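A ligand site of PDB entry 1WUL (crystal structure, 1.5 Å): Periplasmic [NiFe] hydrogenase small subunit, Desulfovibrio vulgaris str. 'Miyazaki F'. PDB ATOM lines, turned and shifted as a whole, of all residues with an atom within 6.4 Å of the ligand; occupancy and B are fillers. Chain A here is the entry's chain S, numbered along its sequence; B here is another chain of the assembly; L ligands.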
ATOM      1  N   ALA A  15      -7.782   4.948  37.674  1.00  0.00           N
ATOM      2  CA  ALA A  15      -7.332   3.762  36.968  1.00  0.00           C
ATOM      3  C   ALA A  15      -6.581   4.251  35.743  1.00  0.00           C
ATOM      4  O   ALA A  15      -7.256   4.641  34.768  1.00  0.00           O
ATOM      5  CB  ALA A  15      -8.522   2.849  36.637  1.00  0.00           C
ATOM      6  N   GLU A  16      -5.249   4.248  35.790  1.00  0.00           N
ATOM      7  CA  GLU A  16      -4.435   4.933  34.788  1.00  0.00           C
ATOM      8  C   GLU A  16      -3.073   4.278  34.695  1.00  0.00           C
ATOM      9  O   GLU A  16      -2.724   3.497  35.573  1.00  0.00           O
ATOM     10  CB  GLU A  16      -4.303   6.410  35.181  1.00  0.00           C
ATOM     11  CG  GLU A  16      -4.049   6.658  36.659  1.00  0.00           C
ATOM     12  CD  GLU A  16      -2.598   6.588  37.094  1.00  0.00           C
ATOM     13  OE1 GLU A  16      -1.697   7.052  36.354  1.00  0.00           O
ATOM     14  OE2 GLU A  16      -2.355   6.099  38.229  1.00  0.00           O
ATOM     15  N   CYS A  17      -2.344   4.613  33.634  1.00  0.00           N
ATOM     16  CA  CYS A  17      -1.029   4.027  33.396  1.00  0.00           C
ATOM     17  C   CYS A  17       0.087   5.033  33.663  1.00  0.00           C
ATOM     18  O   CYS A  17       1.260   4.679  33.558  1.00  0.00           O
ATOM     19  CB  CYS A  17      -0.945   3.498  31.955  1.00  0.00           C
ATOM     20  SG  CYS A  17      -0.638   4.816  30.732  1.00  0.00           S
ATOM     21  N   THR A  18      -0.305   6.265  33.953  1.00  0.00           N
ATOM     22  CA  THR A  18       0.585   7.374  34.309  1.00  0.00           C
ATOM     23  C   THR A  18       1.169   7.962  33.033  1.00  0.00           C
ATOM     24  O   THR A  18       1.963   8.908  33.097  1.00  0.00           O
ATOM     25  CB  THR A  18       1.593   6.989  35.400  1.00  0.00           C
ATOM     26  OG1 THR A  18       0.837   6.471  36.512  1.00  0.00           O
ATOM     27  CG2 THR A  18       2.334   8.197  35.945  1.00  0.00           C
ATOM     28  N   GLY A  19       0.746   7.474  31.864  1.00  0.00           N
ATOM     29  CA  GLY A  19       1.167   8.098  30.594  1.00  0.00           C
ATOM     30  C   GLY A  19       0.671   9.518  30.468  1.00  0.00           C
ATOM     31  O   GLY A  19       1.354  10.388  29.888  1.00  0.00           O
ATOM     32  N   CYS A  20      -0.520   9.813  31.000  1.00  0.00           N
ATOM     33  CA  CYS A  20      -0.964  11.208  30.940  1.00  0.00           C
ATOM     34  C   CYS A  20      -0.129  12.083  31.845  1.00  0.00           C
ATOM     35  O   CYS A  20       0.251  13.204  31.459  1.00  0.00           O
ATOM     36  CB  CYS A  20      -2.457  11.278  31.310  1.00  0.00           C
ATOM     37  SG  CYS A  20      -3.554  10.572  30.015  1.00  0.00           S
ATOM     38  N   SER A  21       0.207  11.646  33.065  1.00  0.00           N
ATOM     39  CA  SER A  21       1.114  12.458  33.886  1.00  0.00           C
ATOM     40  C   SER A  21       2.442  12.684  33.176  1.00  0.00           C
ATOM     41  O   SER A  21       2.980  13.796  33.197  1.00  0.00           O
ATOM     42  CB  SER A  21       1.441  11.765  35.213  1.00  0.00           C
ATOM     43  OG  SER A  21       0.343  11.886  36.091  1.00  0.00           O
ATOM     44  N   GLU A  75      -6.741  12.084  36.101  1.00  0.00           N
ATOM     45  CA  GLU A  75      -6.197  11.100  35.162  1.00  0.00           C
ATOM     46  C   GLU A  75      -6.758   9.731  35.489  1.00  0.00           C
ATOM     47  O   GLU A  75      -6.772   9.356  36.666  1.00  0.00           O
ATOM     48  CB  GLU A  75      -4.661  11.120  35.236  1.00  0.00           C
ATOM     49  CG  GLU A  75      -3.899  10.040  34.457  1.00  0.00           C
ATOM     50  CD  GLU A  75      -2.385  10.262  34.555  1.00  0.00           C
ATOM     51  OE1 GLU A  75      -1.638   9.437  33.963  1.00  0.00           O
ATOM     52  OE2 GLU A  75      -1.964  11.232  35.215  1.00  0.00           O
ATOM     53  N   GLY A  76      -7.241   8.990  34.502  1.00  0.00           N
ATOM     54  CA  GLY A  76      -7.630   7.619  34.703  1.00  0.00           C
ATOM     55  C   GLY A  76      -9.149   7.487  34.839  1.00  0.00           C
ATOM     56  O   GLY A  76      -9.871   8.412  35.260  1.00  0.00           O
ATOM     57  N   GLY A  77      -9.653   6.303  34.483  1.00  0.00           N
ATOM     58  CA  GLY A  77     -11.077   6.005  34.618  1.00  0.00           C
ATOM     59  C   GLY A  77     -11.420   5.651  36.054  1.00  0.00           C
ATOM     60  O   GLY A  77     -10.557   5.285  36.845  1.00  0.00           O
ATOM     61  N   TYR A 111      -8.345  14.486  32.014  1.00  0.00           N
ATOM     62  CA  TYR A 111      -7.186  14.508  31.118  1.00  0.00           C
ATOM     63  C   TYR A 111      -6.835  13.083  30.758  1.00  0.00           C
ATOM     64  O   TYR A 111      -6.505  12.247  31.595  1.00  0.00           O
ATOM     65  CB  TYR A 111      -6.036  15.243  31.806  1.00  0.00           C
ATOM     66  CG  TYR A 111      -4.812  15.384  30.926  1.00  0.00           C
ATOM     67  CD1 TYR A 111      -4.866  16.160  29.763  1.00  0.00           C
ATOM     68  CD2 TYR A 111      -3.606  14.777  31.200  1.00  0.00           C
ATOM     69  CE1 TYR A 111      -3.785  16.323  28.923  1.00  0.00           C
ATOM     70  CE2 TYR A 111      -2.517  14.927  30.373  1.00  0.00           C
ATOM     71  CZ  TYR A 111      -2.575  15.692  29.232  1.00  0.00           C
ATOM     72  OH  TYR A 111      -1.506  15.874  28.371  1.00  0.00           O
ATOM     73  N   GLY A 112      -6.939  12.786  29.446  1.00  0.00           N
ATOM     74  CA  GLY A 112      -6.768  11.359  29.228  1.00  0.00           C
ATOM     75  C   GLY A 112      -8.035  10.724  28.712  1.00  0.00           C
ATOM     76  O   GLY A 112      -9.039  10.934  29.357  1.00  0.00           O
ATOM     77  N   THR A 113      -7.986   9.997  27.578  1.00  0.00           N
ATOM     78  CA  THR A 113      -9.160   9.198  27.182  1.00  0.00           C
ATOM     79  C   THR A 113      -9.705   8.334  28.312  1.00  0.00           C
ATOM     80  O   THR A 113     -10.916   8.075  28.396  1.00  0.00           O
ATOM     81  CB  THR A 113      -8.794   8.342  25.944  1.00  0.00           C
ATOM     82  OG1 THR A 113      -8.568   9.317  24.917  1.00  0.00           O
ATOM     83  CG2 THR A 113      -9.890   7.379  25.471  1.00  0.00           C
ATOM     84  N   CYS A 114      -8.850   7.824  29.209  1.00  0.00           N
ATOM     85  CA  CYS A 114      -9.383   7.070  30.345  1.00  0.00           C
ATOM     86  C   CYS A 114     -10.301   7.940  31.220  1.00  0.00           C
ATOM     87  O   CYS A 114     -11.450   7.568  31.519  1.00  0.00           O
ATOM     88  CB  CYS A 114      -8.296   6.479  31.245  1.00  0.00           C
ATOM     89  SG  CYS A 114      -7.259   5.213  30.466  1.00  0.00           S
ATOM     90  N   ALA A 115      -9.774   9.091  31.667  1.00  0.00           N
ATOM     91  CA  ALA A 115     -10.608  10.001  32.430  1.00  0.00           C
ATOM     92  C   ALA A 115     -11.780  10.552  31.628  1.00  0.00           C
ATOM     93  O   ALA A 115     -12.872  10.728  32.216  1.00  0.00           O
ATOM     94  CB  ALA A 115      -9.767  11.188  32.960  1.00  0.00           C
ATOM     95  N   GLY A 119     -11.558   4.676  28.714  1.00  0.00           N
ATOM     96  CA  GLY A 119     -10.228   4.239  28.327  1.00  0.00           C
ATOM     97  C   GLY A 119     -10.010   2.731  28.346  1.00  0.00           C
ATOM     98  O   GLY A 119     -10.916   1.912  28.241  1.00  0.00           O
ATOM     99  N   VAL A 120      -8.716   2.396  28.487  1.00  0.00           N
ATOM    100  CA  VAL A 120      -8.282   1.035  28.171  1.00  0.00           C
ATOM    101  C   VAL A 120      -8.926   0.027  29.102  1.00  0.00           C
ATOM    102  O   VAL A 120      -9.343  -1.053  28.647  1.00  0.00           O
ATOM    103  CB  VAL A 120      -6.741   0.896  28.138  1.00  0.00           C
ATOM    104  CG1 VAL A 120      -6.115   1.041  29.538  1.00  0.00           C
ATOM    105  CG2 VAL A 120      -6.298  -0.399  27.496  1.00  0.00           C
ATOM    106  N   GLN A 121      -9.065   0.313  30.405  1.00  0.00           N
ATOM    107  CA  GLN A 121      -9.689  -0.675  31.285  1.00  0.00           C
ATOM    108  C   GLN A 121     -11.197  -0.747  31.074  1.00  0.00           C
ATOM    109  O   GLN A 121     -11.845  -1.705  31.537  1.00  0.00           O
ATOM    110  CB  GLN A 121      -9.348  -0.359  32.750  1.00  0.00           C
ATOM    111  CG  GLN A 121      -9.718   1.035  33.224  1.00  0.00           C
ATOM    112  CD  GLN A 121      -8.645   2.060  32.898  1.00  0.00           C
ATOM    113  OE1 GLN A 121      -7.451   1.822  33.111  1.00  0.00           O
ATOM    114  NE2 GLN A 121      -9.043   3.206  32.359  1.00  0.00           N
ATOM    115  N   GLY A 149      -7.225  11.747  24.222  1.00  0.00           N
ATOM    116  CA  GLY A 149      -5.984  11.217  23.664  1.00  0.00           C
ATOM    117  C   GLY A 149      -5.353  10.233  24.655  1.00  0.00           C
ATOM    118  O   GLY A 149      -5.577  10.274  25.863  1.00  0.00           O
ATOM    119  N   CYS A 150      -4.454   9.392  24.185  1.00  0.00           N
ATOM    120  CA  CYS A 150      -3.882   8.321  25.009  1.00  0.00           C
ATOM    121  C   CYS A 150      -2.385   8.229  24.852  1.00  0.00           C
ATOM    122  O   CYS A 150      -1.841   7.276  24.267  1.00  0.00           O
ATOM    123  CB  CYS A 150      -4.613   7.025  24.598  1.00  0.00           C
ATOM    124  SG  CYS A 150      -4.393   5.636  25.760  1.00  0.00           S
ATOM    125  N   PRO A 151      -1.642   9.175  25.430  1.00  0.00           N
ATOM    126  CA  PRO A 151      -2.168  10.354  26.128  1.00  0.00           C
ATOM    127  C   PRO A 151      -2.439  11.548  25.211  1.00  0.00           C
ATOM    128  O   PRO A 151      -2.057  11.531  24.026  1.00  0.00           O
ATOM    129  CB  PRO A 151      -1.009  10.669  27.084  1.00  0.00           C
ATOM    130  CG  PRO A 151       0.238  10.311  26.285  1.00  0.00           C
ATOM    131  CD  PRO A 151      -0.161   9.080  25.501  1.00  0.00           C
ATOM    132  N   PRO A 152      -3.099  12.565  25.727  1.00  0.00           N
ATOM    133  CA  PRO A 152      -3.374  13.761  24.916  1.00  0.00           C
ATOM    134  C   PRO A 152      -2.066  14.513  24.663  1.00  0.00           C
ATOM    135  O   PRO A 152      -1.057  14.258  25.302  1.00  0.00           O
ATOM    136  CB  PRO A 152      -4.281  14.653  25.776  1.00  0.00           C
ATOM    137  CG  PRO A 152      -4.701  13.788  26.925  1.00  0.00           C
ATOM    138  CD  PRO A 152      -3.628  12.745  27.101  1.00  0.00           C
ATOM    139  N   TRP A 258     -10.897   1.655  21.885  1.00  0.00           N
ATOM    140  CA  TRP A 258     -10.353   0.292  21.993  1.00  0.00           C
ATOM    141  C   TRP A 258     -11.314  -0.697  21.346  1.00  0.00           C
ATOM    142  O   TRP A 258     -10.836  -1.710  20.830  1.00  0.00           O
ATOM    143  CB  TRP A 258     -10.123  -0.099  23.463  1.00  0.00           C
ATOM    144  CG  TRP A 258      -9.136   0.858  24.080  1.00  0.00           C
ATOM    145  CD1 TRP A 258      -9.397   1.911  24.913  1.00  0.00           C
ATOM    146  CD2 TRP A 258      -7.729   0.825  23.880  1.00  0.00           C
ATOM    147  NE1 TRP A 258      -8.213   2.528  25.251  1.00  0.00           N
ATOM    148  CE2 TRP A 258      -7.180   1.888  24.630  1.00  0.00           C
ATOM    149  CE3 TRP A 258      -6.894  -0.020  23.118  1.00  0.00           C
ATOM    150  CZ2 TRP A 258      -5.784   2.132  24.652  1.00  0.00           C
ATOM    151  CZ3 TRP A 258      -5.534   0.230  23.150  1.00  0.00           C
ATOM    152  CH2 TRP A 258      -4.992   1.305  23.900  1.00  0.00           C
ATOM    153  N   ARG B  41      -6.760  -3.448  36.730  1.00  0.00           N
ATOM    154  CA  ARG B  41      -7.392  -3.055  35.468  1.00  0.00           C
ATOM    155  C   ARG B  41      -7.826  -4.263  34.666  1.00  0.00           C
ATOM    156  O   ARG B  41      -8.904  -4.249  34.018  1.00  0.00           O
ATOM    157  CB  ARG B  41      -6.475  -2.127  34.636  1.00  0.00           C
ATOM    158  CG  ARG B  41      -6.386  -0.770  35.295  1.00  0.00           C
ATOM    159  CD  ARG B  41      -5.371   0.168  34.640  1.00  0.00           C
ATOM    160  NE  ARG B  41      -4.042  -0.447  34.692  1.00  0.00           N
ATOM    161  CZ  ARG B  41      -3.070  -0.251  33.824  1.00  0.00           C
ATOM    162  NH1 ARG B  41      -3.165   0.579  32.778  1.00  0.00           N
ATOM    163  NH2 ARG B  41      -1.924  -0.932  34.003  1.00  0.00           N
ATOM    164  N   ARG B  61      -0.396   0.367  27.120  1.00  0.00           N
ATOM    165  CA  ARG B  61      -1.098   1.125  28.155  1.00  0.00           C
ATOM    166  C   ARG B  61      -1.060   0.428  29.504  1.00  0.00           C
ATOM    167  O   ARG B  61      -1.693   0.884  30.469  1.00  0.00           O
ATOM    168  CB  ARG B  61      -2.537   1.432  27.699  1.00  0.00           C
ATOM    169  CG  ARG B  61      -2.635   2.619  26.783  1.00  0.00           C
ATOM    170  CD  ARG B  61      -1.907   2.386  25.457  1.00  0.00           C
ATOM    171  NE  ARG B  61      -2.083   3.609  24.646  1.00  0.00           N
ATOM    172  CZ  ARG B  61      -1.618   3.707  23.405  1.00  0.00           C
ATOM    173  NH1 ARG B  61      -0.983   2.665  22.834  1.00  0.00           N
ATOM    174  NH2 ARG B  61      -1.784   4.841  22.728  1.00  0.00           N
ATOM    175  N   CYS B  63       1.606   0.748  31.110  1.00  0.00           N
ATOM    176  CA  CYS B  63       2.395   1.735  31.834  1.00  0.00           C
ATOM    177  C   CYS B  63       2.907   2.826  30.920  1.00  0.00           C
ATOM    178  O   CYS B  63       3.470   2.491  29.841  1.00  0.00           O
ATOM    179  CB  CYS B  63       3.548   0.981  32.502  1.00  0.00           C
ATOM    180  SG  CYS B  63       4.514   2.130  33.560  1.00  0.00           S
ATOM    181  N   GLY B  64       2.746   4.084  31.314  1.00  0.00           N
ATOM    182  CA  GLY B  64       3.225   5.240  30.538  1.00  0.00           C
ATOM    183  C   GLY B  64       4.544   5.756  31.092  1.00  0.00           C
ATOM    184  O   GLY B  64       5.099   6.680  30.515  1.00  0.00           O
ATOM    185  N   PRO B 216       4.735  10.230  25.565  1.00  0.00           N
ATOM    186  CA  PRO B 216       4.558   8.799  25.785  1.00  0.00           C
ATOM    187  C   PRO B 216       3.773   8.066  24.722  1.00  0.00           C
ATOM    188  O   PRO B 216       3.018   8.662  23.938  1.00  0.00           O
ATOM    189  CB  PRO B 216       3.722   8.709  27.090  1.00  0.00           C
ATOM    190  CG  PRO B 216       3.929  10.054  27.732  1.00  0.00           C
ATOM    191  CD  PRO B 216       3.968  11.021  26.563  1.00  0.00           C
ATOM    192  N   HIS B 217       3.953   6.762  24.716  1.00  0.00           N
ATOM    193  CA  HIS B 217       3.266   5.725  23.963  1.00  0.00           C
ATOM    194  C   HIS B 217       3.609   5.788  22.490  1.00  0.00           C
ATOM    195  O   HIS B 217       2.973   6.406  21.648  1.00  0.00           O
ATOM    196  CB  HIS B 217       1.750   5.774  24.178  1.00  0.00           C
ATOM    197  CG  HIS B 217       1.436   5.270  25.576  1.00  0.00           C
ATOM    198  ND1 HIS B 217       0.275   5.445  26.289  1.00  0.00           N
ATOM    199  CD2 HIS B 217       2.273   4.516  26.388  1.00  0.00           C
ATOM    200  CE1 HIS B 217       0.406   4.833  27.489  1.00  0.00           C
ATOM    201  NE2 HIS B 217       1.607   4.272  27.558  1.00  0.00           N
HETATM  202 FE1  LIG L   1      -2.617   5.831  30.128  1.00  0.00          FE
HETATM  203 FE2  LIG L   1      -5.233   6.220  30.131  1.00  0.00          FE
HETATM  204 FE3  LIG L   1      -3.912   6.391  27.882  1.00  0.00          FE
HETATM  205 FE4  LIG L   1      -3.558   8.353  29.743  1.00  0.00          FE
HETATM  206  S1  LIG L   1      -5.473   7.926  28.582  1.00  0.00           S
HETATM  207  S2  LIG L   1      -1.960   7.328  28.482  1.00  0.00           S
HETATM  208  S3  LIG L   1      -3.797   7.094  31.678  1.00  0.00           S
HETATM  209  S4  LIG L   1      -4.123   4.476  29.174  1.00  0.00           S
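FE4 of the ligand is bound by SG of Cys 20, at 2.2 Å. A sulfur (S1) of the ligand lies close to the backbone NH (N) of Cys 114 (3.4 Å). The side-chain sulfur of Cys 114 is bound to an iron atom (FE2) of the ligand, 2.3 Å away. FE3 of the ligand is bound by SG of Cys 150 (2.3 Å). S3 of the ligand sits close to N of Cys 17, at 3.5 Å. The side-chain sulfur (SG) of Cys 17 binds an iron atom (FE1) of the ligand (2.3 Å). S1 of the ligand lies close to N of Thr 113 (3.4 Å). ND1 of His 217 of chain B sits close to S2 of the ligand (3.7 Å).
O of Gly 149 sits close to S1 of the ligand (3.6 Å). N of Pro 151 lies close to S2 of the ligand (3.6 Å). Glu 16 touches the ligand (CB to S3, 3.6 Å). CA of Gly 19 touches S2 of the ligand, at 3.9 Å. OE1 of Glu 75 touches S3 of the ligand, at 3.9 Å. CA of Gly 112 touches S1 of the ligand (3.7 Å). Val 120 touches the ligand. Arg 61 of chain B touches the ligand. Hydrophobic or aromatic side chains within 4 Å of the ligand: Val 120, Pro 151 and His 217 of chain B. Within 4 Å of the ligand: Glu 16, Cys 17, Gly 19, Cys 20, Glu 75, Gly 112, Thr 113, Cys 114, Val 120, Gly 149, Cys 150, Pro 151, Arg 61 of chain B and His 217 of chain B. The nearest printed residue that does not touch the ligand is Thr 18 (4.2 Å).
SG of Cys 20 lies close to O of Tyr 111 (3.7 Å). N of Val 120 sits close to SG of Cys 114, 3.7 Å away. The backbone carbonyl oxygen (O) of Cys 150 sits at hydrogen-bond distance from a ring nitrogen (ND1) of His 217 of chain B, 3.5 Å away. The side-chain sulfur (SG) of Cys 17 sits close to the backbone NH (N) of Gly 19, at 3.2 Å. O of Cys 17 sits at hydrogen-bond distance from N of Gly 64 of chain B (2.8 Å). The side-chain hydroxyl (OG1) of Thr 113 sits at hydrogen-bond distance from the backbone NH (N) of Gly 149 (2.9 Å). O of Thr 113 sits at hydrogen-bond distance from N of Gly 119. OE2 of Glu 75 is in hydrogen-bond range of OG of Ser 21 (2.6 Å).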
